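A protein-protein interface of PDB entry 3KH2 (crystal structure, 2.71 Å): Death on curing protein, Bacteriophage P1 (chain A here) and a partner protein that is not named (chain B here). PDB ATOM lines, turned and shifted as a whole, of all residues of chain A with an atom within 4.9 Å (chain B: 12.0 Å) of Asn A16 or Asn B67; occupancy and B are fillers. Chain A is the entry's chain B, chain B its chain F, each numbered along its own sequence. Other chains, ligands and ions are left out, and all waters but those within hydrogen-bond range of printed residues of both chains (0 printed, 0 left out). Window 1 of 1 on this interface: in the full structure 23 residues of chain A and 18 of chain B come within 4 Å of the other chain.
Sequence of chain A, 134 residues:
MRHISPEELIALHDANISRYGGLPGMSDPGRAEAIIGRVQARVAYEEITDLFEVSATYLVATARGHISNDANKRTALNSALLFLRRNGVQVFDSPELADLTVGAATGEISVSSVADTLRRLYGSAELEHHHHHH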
ATOM      1  N   LEU A  12      23.163  14.965   5.487  1.00  0.00           N
ATOM      2  CA  LEU A  12      22.455  15.551   6.626  1.00  0.00           C
ATOM      3  C   LEU A  12      23.253  15.357   7.906  1.00  0.00           C
ATOM      4  O   LEU A  12      23.402  16.271   8.713  1.00  0.00           O
ATOM      5  CB  LEU A  12      21.074  14.901   6.768  1.00  0.00           C
ATOM      6  CG  LEU A  12      20.152  15.328   7.915  1.00  0.00           C
ATOM      7  CD1 LEU A  12      19.899  16.830   7.944  1.00  0.00           C
ATOM      8  CD2 LEU A  12      18.830  14.572   7.782  1.00  0.00           C
ATOM      9  N   HIS A  13      23.771  14.152   8.074  1.00  0.00           N
ATOM     10  CA  HIS A  13      24.608  13.812   9.223  1.00  0.00           C
ATOM     11  C   HIS A  13      25.885  14.665   9.270  1.00  0.00           C
ATOM     12  O   HIS A  13      26.223  15.230  10.323  1.00  0.00           O
ATOM     13  CB  HIS A  13      24.964  12.328   9.152  1.00  0.00           C
ATOM     14  CG  HIS A  13      25.676  11.813  10.358  1.00  0.00           C
ATOM     15  ND1 HIS A  13      25.023  11.155  11.374  1.00  0.00           N
ATOM     16  CD2 HIS A  13      26.984  11.839  10.702  1.00  0.00           C
ATOM     17  CE1 HIS A  13      25.900  10.797  12.297  1.00  0.00           C
ATOM     18  NE2 HIS A  13      27.098  11.202  11.916  1.00  0.00           N
ATOM     19  N   ASP A  14      26.593  14.751   8.138  1.00  0.00           N
ATOM     20  CA  ASP A  14      27.829  15.562   8.057  1.00  0.00           C
ATOM     21  C   ASP A  14      27.556  17.034   8.311  1.00  0.00           C
ATOM     22  O   ASP A  14      28.323  17.694   9.000  1.00  0.00           O
ATOM     23  CB  ASP A  14      28.530  15.402   6.708  1.00  0.00           C
ATOM     24  CG  ASP A  14      29.154  14.024   6.530  1.00  0.00           C
ATOM     25  OD1 ASP A  14      29.223  13.256   7.521  1.00  0.00           O
ATOM     26  OD2 ASP A  14      29.570  13.710   5.387  1.00  0.00           O
ATOM     27  N   ALA A  15      26.455  17.535   7.761  1.00  0.00           N
ATOM     28  CA  ALA A  15      26.062  18.929   7.947  1.00  0.00           C
ATOM     29  C   ALA A  15      25.761  19.217   9.414  1.00  0.00           C
ATOM     30  O   ALA A  15      26.077  20.291   9.932  1.00  0.00           O
ATOM     31  CB  ALA A  15      24.856  19.249   7.096  1.00  0.00           C
ATOM     32  N   ASN A  16      25.158  18.246  10.086  1.00  0.00           N
ATOM     33  CA  ASN A  16      24.777  18.411  11.479  1.00  0.00           C
ATOM     34  C   ASN A  16      25.998  18.398  12.394  1.00  0.00           C
ATOM     35  O   ASN A  16      26.070  19.166  13.353  1.00  0.00           O
ATOM     36  CB  ASN A  16      23.784  17.324  11.884  1.00  0.00           C
ATOM     37  CG  ASN A  16      23.281  17.499  13.296  1.00  0.00           C
ATOM     38  OD1 ASN A  16      23.987  17.196  14.260  1.00  0.00           O
ATOM     39  ND2 ASN A  16      22.048  17.993  13.433  1.00  0.00           N
ATOM     40  N   ILE A  17      26.952  17.517  12.098  1.00  0.00           N
ATOM     41  CA  ILE A  17      28.175  17.429  12.886  1.00  0.00           C
ATOM     42  C   ILE A  17      28.980  18.720  12.768  1.00  0.00           C
ATOM     43  O   ILE A  17      29.500  19.218  13.764  1.00  0.00           O
ATOM     44  CB  ILE A  17      29.039  16.227  12.471  1.00  0.00           C
ATOM     45  CG1 ILE A  17      28.404  14.922  12.975  1.00  0.00           C
ATOM     46  CG2 ILE A  17      30.436  16.360  13.035  1.00  0.00           C
ATOM     47  CD1 ILE A  17      29.178  13.659  12.617  1.00  0.00           C
ATOM     48  N   SER A  18      29.070  19.262  11.557  1.00  0.00           N
ATOM     49  CA  SER A  18      29.750  20.530  11.333  1.00  0.00           C
ATOM     50  C   SER A  18      29.150  21.633  12.193  1.00  0.00           C
ATOM     51  O   SER A  18      29.875  22.375  12.856  1.00  0.00           O
ATOM     52  CB  SER A  18      29.652  20.944   9.866  1.00  0.00           C
ATOM     53  OG  SER A  18      30.366  20.051   9.044  1.00  0.00           O
ATOM     54  N   ARG A  19      27.823  21.733  12.181  1.00  0.00           N
ATOM     55  CA  ARG A  19      27.137  22.873  12.791  1.00  0.00           C
ATOM     56  C   ARG A  19      27.052  22.806  14.322  1.00  0.00           C
ATOM     57  O   ARG A  19      27.265  23.818  15.006  1.00  0.00           O
ATOM     58  CB  ARG A  19      25.737  23.024  12.199  1.00  0.00           C
ATOM     59  CG  ARG A  19      24.912  24.116  12.858  1.00  0.00           C
ATOM     60  CD  ARG A  19      23.791  24.607  11.954  1.00  0.00           C
ATOM     61  NE  ARG A  19      22.857  25.472  12.677  1.00  0.00           N
ATOM     62  CZ  ARG A  19      21.947  26.259  12.105  1.00  0.00           C
ATOM     63  NH1 ARG A  19      21.819  26.314  10.780  1.00  0.00           N
ATOM     64  NH2 ARG A  19      21.148  26.992  12.871  1.00  0.00           N
ATOM     65  N   TYR A  20      26.748  21.620  14.847  1.00  0.00           N
ATOM     66  CA  TYR A  20      26.437  21.451  16.270  1.00  0.00           C
ATOM     67  C   TYR A  20      27.501  20.713  17.090  1.00  0.00           C
ATOM     68  O   TYR A  20      27.564  20.891  18.309  1.00  0.00           O
ATOM     69  CB  TYR A  20      25.086  20.755  16.416  1.00  0.00           C
ATOM     70  CG  TYR A  20      23.941  21.590  15.905  1.00  0.00           C
ATOM     71  CD1 TYR A  20      23.431  22.641  16.658  1.00  0.00           C
ATOM     72  CD2 TYR A  20      23.375  21.346  14.654  1.00  0.00           C
ATOM     73  CE1 TYR A  20      22.377  23.424  16.184  1.00  0.00           C
ATOM     74  CE2 TYR A  20      22.322  22.121  14.174  1.00  0.00           C
ATOM     75  CZ  TYR A  20      21.831  23.155  14.943  1.00  0.00           C
ATOM     76  OH  TYR A  20      20.797  23.924  14.478  1.00  0.00           O
ATOM     77  N   GLY A  21      28.308  19.876  16.436  1.00  0.00           N
ATOM     78  CA  GLY A  21      29.424  19.187  17.102  1.00  0.00           C
ATOM     79  C   GLY A  21      29.467  17.689  16.850  1.00  0.00           C
ATOM     80  O   GLY A  21      28.491  17.103  16.381  1.00  0.00           O
ATOM     81  N   ALA A  71      26.196  11.839  16.952  1.00  0.00           N
ATOM     82  CA  ALA A  71      25.122  12.637  16.325  1.00  0.00           C
ATOM     83  C   ALA A  71      23.975  11.840  15.688  1.00  0.00           C
ATOM     84  O   ALA A  71      23.255  12.372  14.836  1.00  0.00           O
ATOM     85  CB  ALA A  71      25.715  13.614  15.301  1.00  0.00           C
ATOM     86  N   ARG A  74      20.445  13.235  16.611  1.00  0.00           N
ATOM     87  CA  ARG A  74      20.168  14.447  15.827  1.00  0.00           C
ATOM     88  C   ARG A  74      19.779  14.132  14.383  1.00  0.00           C
ATOM     89  O   ARG A  74      18.810  14.683  13.869  1.00  0.00           O
ATOM     90  CB  ARG A  74      21.364  15.401  15.852  1.00  0.00           C
ATOM     91  CG  ARG A  74      21.429  16.249  17.110  1.00  0.00           C
ATOM     92  CD  ARG A  74      22.725  17.015  17.187  1.00  0.00           C
ATOM     93  NE  ARG A  74      23.825  16.156  17.606  1.00  0.00           N
ATOM     94  CZ  ARG A  74      25.104  16.335  17.285  1.00  0.00           C
ATOM     95  NH1 ARG A  74      25.478  17.343  16.508  1.00  0.00           N
ATOM     96  NH2 ARG A  74      26.021  15.491  17.743  1.00  0.00           N
ATOM     97  N   ASN A  78      16.123  15.050  12.818  1.00  0.00           N
ATOM     98  CA  ASN A  78      16.085  15.909  11.648  1.00  0.00           C
ATOM     99  C   ASN A  78      15.591  15.174  10.402  1.00  0.00           C
ATOM    100  O   ASN A  78      14.830  15.724   9.613  1.00  0.00           O
ATOM    101  CB  ASN A  78      17.462  16.508  11.400  1.00  0.00           C
ATOM    102  CG  ASN A  78      17.862  17.489  12.486  1.00  0.00           C
ATOM    103  OD1 ASN A  78      17.172  18.483  12.719  1.00  0.00           O
ATOM    104  ND2 ASN A  78      18.981  17.218  13.157  1.00  0.00           N
ATOM    105  N   LYS B  49      23.218  20.610  -4.835  1.00  0.00           N
ATOM    106  CA  LYS B  49      23.860  20.587  -3.519  1.00  0.00           C
ATOM    107  C   LYS B  49      23.645  21.891  -2.771  1.00  0.00           C
ATOM    108  O   LYS B  49      23.519  21.898  -1.548  1.00  0.00           O
ATOM    109  CB  LYS B  49      25.358  20.312  -3.653  1.00  0.00           C
ATOM    110  CG  LYS B  49      26.138  20.440  -2.342  1.00  0.00           C
ATOM    111  CD  LYS B  49      27.561  19.927  -2.495  1.00  0.00           C
ATOM    112  CE  LYS B  49      28.490  20.487  -1.413  1.00  0.00           C
ATOM    113  NZ  LYS B  49      27.859  20.525  -0.060  1.00  0.00           N
ATOM    114  N   LEU B  52      19.970  21.483  -1.480  1.00  0.00           N
ATOM    115  CA  LEU B  52      19.992  20.572  -0.336  1.00  0.00           C
ATOM    116  C   LEU B  52      20.632  21.217   0.899  1.00  0.00           C
ATOM    117  O   LEU B  52      20.091  21.118   2.004  1.00  0.00           O
ATOM    118  CB  LEU B  52      20.741  19.292  -0.703  1.00  0.00           C
ATOM    119  CG  LEU B  52      20.570  18.118   0.258  1.00  0.00           C
ATOM    120  CD1 LEU B  52      19.104  17.742   0.407  1.00  0.00           C
ATOM    121  CD2 LEU B  52      21.391  16.929  -0.227  1.00  0.00           C
ATOM    122  N   ASP B  53      21.780  21.873   0.712  1.00  0.00           N
ATOM    123  CA  ASP B  53      22.442  22.582   1.809  1.00  0.00           C
ATOM    124  C   ASP B  53      21.517  23.621   2.427  1.00  0.00           C
ATOM    125  O   ASP B  53      21.500  23.779   3.643  1.00  0.00           O
ATOM    126  CB  ASP B  53      23.741  23.261   1.346  1.00  0.00           C
ATOM    127  CG  ASP B  53      24.911  22.278   1.190  1.00  0.00           C
ATOM    128  OD1 ASP B  53      24.750  21.085   1.532  1.00  0.00           O
ATOM    129  OD2 ASP B  53      26.000  22.703   0.723  1.00  0.00           O
ATOM    130  N   ALA B  54      20.753  24.321   1.592  1.00  0.00           N
ATOM    131  CA  ALA B  54      19.854  25.385   2.067  1.00  0.00           C
ATOM    132  C   ALA B  54      18.712  24.779   2.866  1.00  0.00           C
ATOM    133  O   ALA B  54      18.291  25.320   3.898  1.00  0.00           O
ATOM    134  CB  ALA B  54      19.307  26.180   0.897  1.00  0.00           C
ATOM    135  N   GLU B  55      18.231  23.647   2.360  1.00  0.00           N
ATOM    136  CA  GLU B  55      17.151  22.879   2.965  1.00  0.00           C
ATOM    137  C   GLU B  55      17.533  22.474   4.388  1.00  0.00           C
ATOM    138  O   GLU B  55      16.744  22.635   5.318  1.00  0.00           O
ATOM    139  CB  GLU B  55      16.854  21.643   2.094  1.00  0.00           C
ATOM    140  CG  GLU B  55      15.538  20.923   2.388  1.00  0.00           C
ATOM    141  CD  GLU B  55      15.249  19.757   1.421  1.00  0.00           C
ATOM    142  OE1 GLU B  55      16.081  19.457   0.526  1.00  0.00           O
ATOM    143  OE2 GLU B  55      14.170  19.136   1.562  1.00  0.00           O
ATOM    144  N   PHE B  56      18.759  21.975   4.545  1.00  0.00           N
ATOM    145  CA  PHE B  56      19.271  21.576   5.859  1.00  0.00           C
ATOM    146  C   PHE B  56      19.415  22.759   6.803  1.00  0.00           C
ATOM    147  O   PHE B  56      19.168  22.636   7.999  1.00  0.00           O
ATOM    148  CB  PHE B  56      20.635  20.883   5.757  1.00  0.00           C
ATOM    149  CG  PHE B  56      20.617  19.559   5.046  1.00  0.00           C
ATOM    150  CD1 PHE B  56      19.443  18.835   4.867  1.00  0.00           C
ATOM    151  CD2 PHE B  56      21.804  19.018   4.586  1.00  0.00           C
ATOM    152  CE1 PHE B  56      19.456  17.614   4.205  1.00  0.00           C
ATOM    153  CE2 PHE B  56      21.829  17.798   3.932  1.00  0.00           C
ATOM    154  CZ  PHE B  56      20.652  17.093   3.739  1.00  0.00           C
ATOM    155  N   ALA B  57      19.838  23.893   6.263  1.00  0.00           N
ATOM    156  CA  ALA B  57      19.979  25.107   7.051  1.00  0.00           C
ATOM    157  C   ALA B  57      18.649  25.511   7.699  1.00  0.00           C
ATOM    158  O   ALA B  57      18.619  25.837   8.884  1.00  0.00           O
ATOM    159  CB  ALA B  57      20.532  26.232   6.193  1.00  0.00           C
ATOM    160  N   SER B  58      17.552  25.464   6.940  1.00  0.00           N
ATOM    161  CA  SER B  58      16.237  25.846   7.480  1.00  0.00           C
ATOM    162  C   SER B  58      15.755  24.842   8.510  1.00  0.00           C
ATOM    163  O   SER B  58      15.248  25.230   9.567  1.00  0.00           O
ATOM    164  CB  SER B  58      15.183  25.968   6.387  1.00  0.00           C
ATOM    165  OG  SER B  58      15.766  26.441   5.203  1.00  0.00           O
ATOM    166  N   LEU B  59      15.905  23.560   8.201  1.00  0.00           N
ATOM    167  CA  LEU B  59      15.532  22.512   9.143  1.00  0.00           C
ATOM    168  C   LEU B  59      16.255  22.737  10.476  1.00  0.00           C
ATOM    169  O   LEU B  59      15.619  22.762  11.530  1.00  0.00           O
ATOM    170  CB  LEU B  59      15.848  21.125   8.575  1.00  0.00           C
ATOM    171  CG  LEU B  59      15.291  19.922   9.351  1.00  0.00           C
ATOM    172  CD1 LEU B  59      13.772  19.885   9.363  1.00  0.00           C
ATOM    173  CD2 LEU B  59      15.833  18.643   8.765  1.00  0.00           C
ATOM    174  N   PHE B  60      17.571  22.946  10.407  1.00  0.00           N
ATOM    175  CA  PHE B  60      18.404  23.181  11.589  1.00  0.00           C
ATOM    176  C   PHE B  60      18.052  24.465  12.329  1.00  0.00           C
ATOM    177  O   PHE B  60      18.076  24.488  13.564  1.00  0.00           O
ATOM    178  CB  PHE B  60      19.895  23.204  11.223  1.00  0.00           C
ATOM    179  CG  PHE B  60      20.442  21.881  10.732  1.00  0.00           C
ATOM    180  CD1 PHE B  60      19.808  20.667  11.014  1.00  0.00           C
ATOM    181  CD2 PHE B  60      21.621  21.851  10.001  1.00  0.00           C
ATOM    182  CE1 PHE B  60      20.331  19.464  10.553  1.00  0.00           C
ATOM    183  CE2 PHE B  60      22.152  20.646   9.542  1.00  0.00           C
ATOM    184  CZ  PHE B  60      21.505  19.454   9.821  1.00  0.00           C
ATOM    185  N   ASP B  61      17.742  25.530  11.590  1.00  0.00           N
ATOM    186  CA  ASP B  61      17.263  26.783  12.206  1.00  0.00           C
ATOM    187  C   ASP B  61      15.960  26.560  12.969  1.00  0.00           C
ATOM    188  O   ASP B  61      15.807  27.007  14.100  1.00  0.00           O
ATOM    189  CB  ASP B  61      17.027  27.862  11.146  1.00  0.00           C
ATOM    190  CG  ASP B  61      18.311  28.430  10.586  1.00  0.00           C
ATOM    191  OD1 ASP B  61      19.377  27.819  10.796  1.00  0.00           O
ATOM    192  OD2 ASP B  61      18.250  29.488   9.929  1.00  0.00           O
ATOM    193  N   THR B  62      15.023  25.874  12.326  1.00  0.00           N
ATOM    194  CA  THR B  62      13.734  25.559  12.933  1.00  0.00           C
ATOM    195  C   THR B  62      13.907  24.722  14.206  1.00  0.00           C
ATOM    196  O   THR B  62      13.215  24.952  15.194  1.00  0.00           O
ATOM    197  CB  THR B  62      12.821  24.809  11.935  1.00  0.00           C
ATOM    198  OG1 THR B  62      12.618  25.612  10.767  1.00  0.00           O
ATOM    199  CG2 THR B  62      11.473  24.478  12.565  1.00  0.00           C
ATOM    200  N   LEU B  63      14.845  23.775  14.177  1.00  0.00           N
ATOM    201  CA  LEU B  63      15.061  22.850  15.290  1.00  0.00           C
ATOM    202  C   LEU B  63      16.346  23.135  16.087  1.00  0.00           C
ATOM    203  O   LEU B  63      16.937  22.220  16.655  1.00  0.00           O
ATOM    204  CB  LEU B  63      15.084  21.412  14.759  1.00  0.00           C
ATOM    205  CG  LEU B  63      13.851  20.968  13.979  1.00  0.00           C
ATOM    206  CD1 LEU B  63      14.043  19.581  13.446  1.00  0.00           C
ATOM    207  CD2 LEU B  63      12.619  21.031  14.857  1.00  0.00           C
ATOM    208  N   ASP B  64      16.736  24.406  16.168  1.00  0.00           N
ATOM    209  CA  ASP B  64      18.037  24.817  16.725  1.00  0.00           C
ATOM    210  C   ASP B  64      18.215  24.481  18.213  1.00  0.00           C
ATOM    211  O   ASP B  64      19.273  23.998  18.622  1.00  0.00           O
ATOM    212  CB  ASP B  64      18.245  26.322  16.503  1.00  0.00           C
ATOM    213  CG  ASP B  64      19.717  26.733  16.530  1.00  0.00           C
ATOM    214  OD1 ASP B  64      20.555  26.112  15.831  1.00  0.00           O
ATOM    215  OD2 ASP B  64      20.032  27.709  17.241  1.00  0.00           O
ATOM    216  N   SER B  65      17.179  24.731  19.013  1.00  0.00           N
ATOM    217  CA  SER B  65      17.222  24.474  20.462  1.00  0.00           C
ATOM    218  C   SER B  65      17.427  23.001  20.784  1.00  0.00           C
ATOM    219  O   SER B  65      18.336  22.639  21.536  1.00  0.00           O
ATOM    220  CB  SER B  65      15.929  24.931  21.137  1.00  0.00           C
ATOM    221  OG  SER B  65      15.750  26.322  21.008  1.00  0.00           O
ATOM    222  N   THR B  66      16.564  22.161  20.224  1.00  0.00           N
ATOM    223  CA  THR B  66      16.606  20.728  20.479  1.00  0.00           C
ATOM    224  C   THR B  66      17.875  20.090  19.905  1.00  0.00           C
ATOM    225  O   THR B  66      18.425  19.160  20.491  1.00  0.00           O
ATOM    226  CB  THR B  66      15.355  20.055  19.922  1.00  0.00           C
ATOM    227  OG1 THR B  66      14.209  20.569  20.615  1.00  0.00           O
ATOM    228  CG2 THR B  66      15.420  18.543  20.090  1.00  0.00           C
ATOM    229  N   ASN B  67      18.342  20.608  18.771  1.00  0.00           N
ATOM    230  CA  ASN B  67      19.610  20.164  18.203  1.00  0.00           C
ATOM    231  C   ASN B  67      20.757  20.454  19.169  1.00  0.00           C
ATOM    232  O   ASN B  67      21.570  19.574  19.432  1.00  0.00           O
ATOM    233  CB  ASN B  67      19.867  20.800  16.828  1.00  0.00           C
ATOM    234  CG  ASN B  67      19.314  19.964  15.670  1.00  0.00           C
ATOM    235  OD1 ASN B  67      19.711  18.819  15.468  1.00  0.00           O
ATOM    236  ND2 ASN B  67      18.420  20.547  14.892  1.00  0.00           N
ATOM    237  N   LYS B  68      20.808  21.671  19.708  1.00  0.00           N
ATOM    238  CA  LYS B  68      21.836  22.039  20.704  1.00  0.00           C
ATOM    239  C   LYS B  68      21.763  21.160  21.949  1.00  0.00           C
ATOM    240  O   LYS B  68      22.788  20.746  22.492  1.00  0.00           O
ATOM    241  CB  LYS B  68      21.710  23.507  21.127  1.00  0.00           C
ATOM    242  CG  LYS B  68      22.286  24.502  20.138  1.00  0.00           C
ATOM    243  CD  LYS B  68      21.843  25.927  20.480  1.00  0.00           C
ATOM    244  CE  LYS B  68      22.232  26.950  19.402  1.00  0.00           C
ATOM    245  NZ  LYS B  68      23.484  27.686  19.712  1.00  0.00           N
ATOM    246  N   GLU B  69      20.546  20.875  22.389  1.00  0.00           N
ATOM    247  CA  GLU B  69      20.328  20.084  23.597  1.00  0.00           C
ATOM    248  C   GLU B  69      20.787  18.634  23.430  1.00  0.00           C
ATOM    249  O   GLU B  69      21.492  18.101  24.287  1.00  0.00           O
ATOM    250  CB  GLU B  69      18.848  20.127  23.979  1.00  0.00           C
ATOM    251  CG  GLU B  69      18.527  19.563  25.357  1.00  0.00           C
ATOM    252  CD  GLU B  69      17.041  19.650  25.680  1.00  0.00           C
ATOM    253  OE1 GLU B  69      16.468  18.628  26.132  1.00  0.00           O
ATOM    254  OE2 GLU B  69      16.450  20.737  25.465  1.00  0.00           O
ATOM    255  N   LEU B  70      20.395  18.009  22.321  1.00  0.00           N
ATOM    256  CA  LEU B  70      20.717  16.604  22.049  1.00  0.00           C
ATOM    257  C   LEU B  70      22.218  16.302  22.031  1.00  0.00           C
ATOM    258  O   LEU B  70      22.622  15.159  22.239  1.00  0.00           O
ATOM    259  CB  LEU B  70      20.086  16.159  20.731  1.00  0.00           C
ATOM    260  CG  LEU B  70      18.564  16.015  20.759  1.00  0.00           C
ATOM    261  CD1 LEU B  70      18.025  15.807  19.360  1.00  0.00           C
ATOM    262  CD2 LEU B  70      18.125  14.882  21.662  1.00  0.00           C
ATOM    263  N   VAL B  71      23.041  17.319  21.785  1.00  0.00           N
ATOM    264  CA  VAL B  71      24.492  17.159  21.844  1.00  0.00           C
ATOM    265  C   VAL B  71      24.936  16.661  23.221  1.00  0.00           C
ATOM    266  O   VAL B  71      25.851  15.845  23.321  1.00  0.00           O
ATOM    267  CB  VAL B  71      25.230  18.476  21.523  1.00  0.00           C
ATOM    268  CG1 VAL B  71      26.722  18.293  21.655  1.00  0.00           C
ATOM    269  CG2 VAL B  71      24.890  18.947  20.133  1.00  0.00           C
ATOM    270  N   ASN B  72      24.267  17.139  24.267  1.00  0.00           N
ATOM    271  CA  ASN B  72      24.658  16.864  25.655  1.00  0.00           C
ATOM    272  C   ASN B  72      23.840  15.776  26.361  1.00  0.00           C
ATOM    273  O   ASN B  72      23.857  15.688  27.587  1.00  0.00           O
ATOM    274  CB  ASN B  72      24.582  18.162  26.472  1.00  0.00           C
ATOM    275  CG  ASN B  72      25.555  19.221  25.984  1.00  0.00           C
ATOM    276  OD1 ASN B  72      26.735  18.943  25.753  1.00  0.00           O
ATOM    277  ND2 ASN B  72      25.066  20.447  25.836  1.00  0.00           N
ATOM    278  N   ARG B  73      23.133  14.949  25.595  1.00  0.00           N
ATOM    279  CA  ARG B  73      22.330  13.856  26.159  1.00  0.00           C
ATOM    280  C   ARG B  73      23.014  12.506  25.940  1.00  0.00           C
ATOM    281  O   ARG B  73      23.636  11.935  26.847  1.00  0.00           O
ATOM    282  CB  ARG B  73      20.943  13.823  25.515  1.00  0.00           C
ATOM    283  CG  ARG B  73      20.044  14.976  25.889  1.00  0.00           C
ATOM    284  CD  ARG B  73      19.460  14.821  27.275  1.00  0.00           C
ATOM    285  NE  ARG B  73      18.211  15.572  27.385  1.00  0.00           N
ATOM    286  CZ  ARG B  73      16.983  15.047  27.374  1.00  0.00           C
ATOM    287  NH1 ARG B  73      16.788  13.732  27.280  1.00  0.00           N
ATOM    288  NH2 ARG B  73      15.931  15.855  27.471  1.00  0.00           N
ATOM    289  OXT ARG B  73      22.955  11.957  24.835  1.00  0.00           O
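The side-chain amide nitrogen (ND2) of Asn A16 sits close to the side-chain amide nitrogen (ND2) of Asn A78 (3.2 Å).
The backbone carbonyl oxygen (O) of Arg A74 lies within hydrogen-bond range of the side-chain amide nitrogen (ND2) of Asn A78 (2.6 Å).
OH of Tyr A20 lies within hydrogen-bond range of NE of Arg A19 (3.1 Å).
The backbone carbonyl oxygen (O) of Gly A21 sits at hydrogen-bond distance from the guanidinium group (NH1) of Arg A74, 3.0 Å away.
The backbone carbonyl oxygen of Leu B63 lies within hydrogen-bond range of the side-chain amide nitrogen of Asn B67 (2.8 Å).
The side-chain amide oxygen (OD1) of Asn A16 lies within hydrogen-bond range of the guanidinium group (NH1) of Arg A74 (2.7 Å).
OD1 of Asn B67 sits at hydrogen-bond distance from ND2 of Asn A16 (3.2 Å).
The side-chain amide oxygen (OD1) of Asn B67 sits at hydrogen-bond distance from the side-chain amide nitrogen (ND2) of Asn A78 (2.9 Å).
The guanidinium group (NH2) of Arg A19 lies within salt-bridge range of the side-chain carboxylate (OD1) of Asp B64, 3.1 Å away.
OH of Tyr A20 is in hydrogen-bond range of OD1 of Asp B64 (2.6 Å).
The guanidinium group (NH2) of Arg A19 is in salt-bridge range of the side-chain carboxylate (OD1) of Asp B61, 2.9 Å away.
OH of Tyr A20 lies within hydrogen-bond range of O of Phe B60.
Among the printed residues, merely in contact across the chains: Leu A12 with Phe B56 (3.5 Å), Leu A12 with Phe B60 (3.6 Å), Ala A15 with Phe B56 (3.96 Å), Ala A15 with Phe B60 (3.9 Å), Asn A16 with Phe B60 (3.7 Å), Arg A19 with Ala B57 (3.7 Å), Arg A19 with Phe B60 (3.7 Å), Tyr A20 with Asn B67 (3.6 Å), Tyr A20 with Val B71 (3.8 Å), Arg A74 with Asn B67 (3.5 Å), Arg A74 with Leu B70 (3.9 Å), Arg A74 with Val B71 (3.9 Å), Asn A78 with Leu B59 (3.2 Å), Asn A78 with Phe B60 (3.7 Å) and Asn A78 with Leu B63 (3.4 Å).
Of the 23 printed residues of chain B, 10 touch a printed residue of chain A.
Of the 13 printed residues of chain A, 7 touch a printed residue of chain B.
Along chain A the printed residues that touch a printed residue of chain B span positions 12 to 78.
Among the printed residues, 21 pairs touch across the chains.
Among the printed residues, Asp or Glu carboxylates within 4 Å of a Lys or Arg side-chain nitrogen of the other chain: Arg A19 with Asp B61 and Arg A19 with Asp B64.
No residue of chain B comes within 4 Å of Asp A14.
Ala A15 touches two residues of chain B.
Of chain B, only Phe B60 (3.7 Å) and Asn B67 (3.2 Å) come within 4 Å of Asn A16.
Ile A17 touches none of the printed residues of chain B.
No residue of chain B comes within 4 Å of Ser A18.
Arg A19 touches just these residues of chain B: Ala B57 (3.7 Å), Phe B60 (3.7 Å), Asp B61 (2.9 Å) and Asp B64 (3.1 Å).
Of chain B, only Phe B60, Asp B64, Asn B67 and Val B71 come within 4 Å of Tyr A20.
No residue of chain B comes within 4 Å of Gly A21.
Ala A71 touches none of the printed residues of chain B.
Of the printed residues of chain A, Leu B59 touches Asn A78.
Printed residues of chain A within 4 Å of Leu B63: Asn A78.
Of the printed residues of chain A, Val B71 touches Tyr A20 (3.8 Å) and Arg A74 (3.9 Å).
The nearest residue of chain B that does not touch Asn A16 is Val B71 (6.2 Å).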
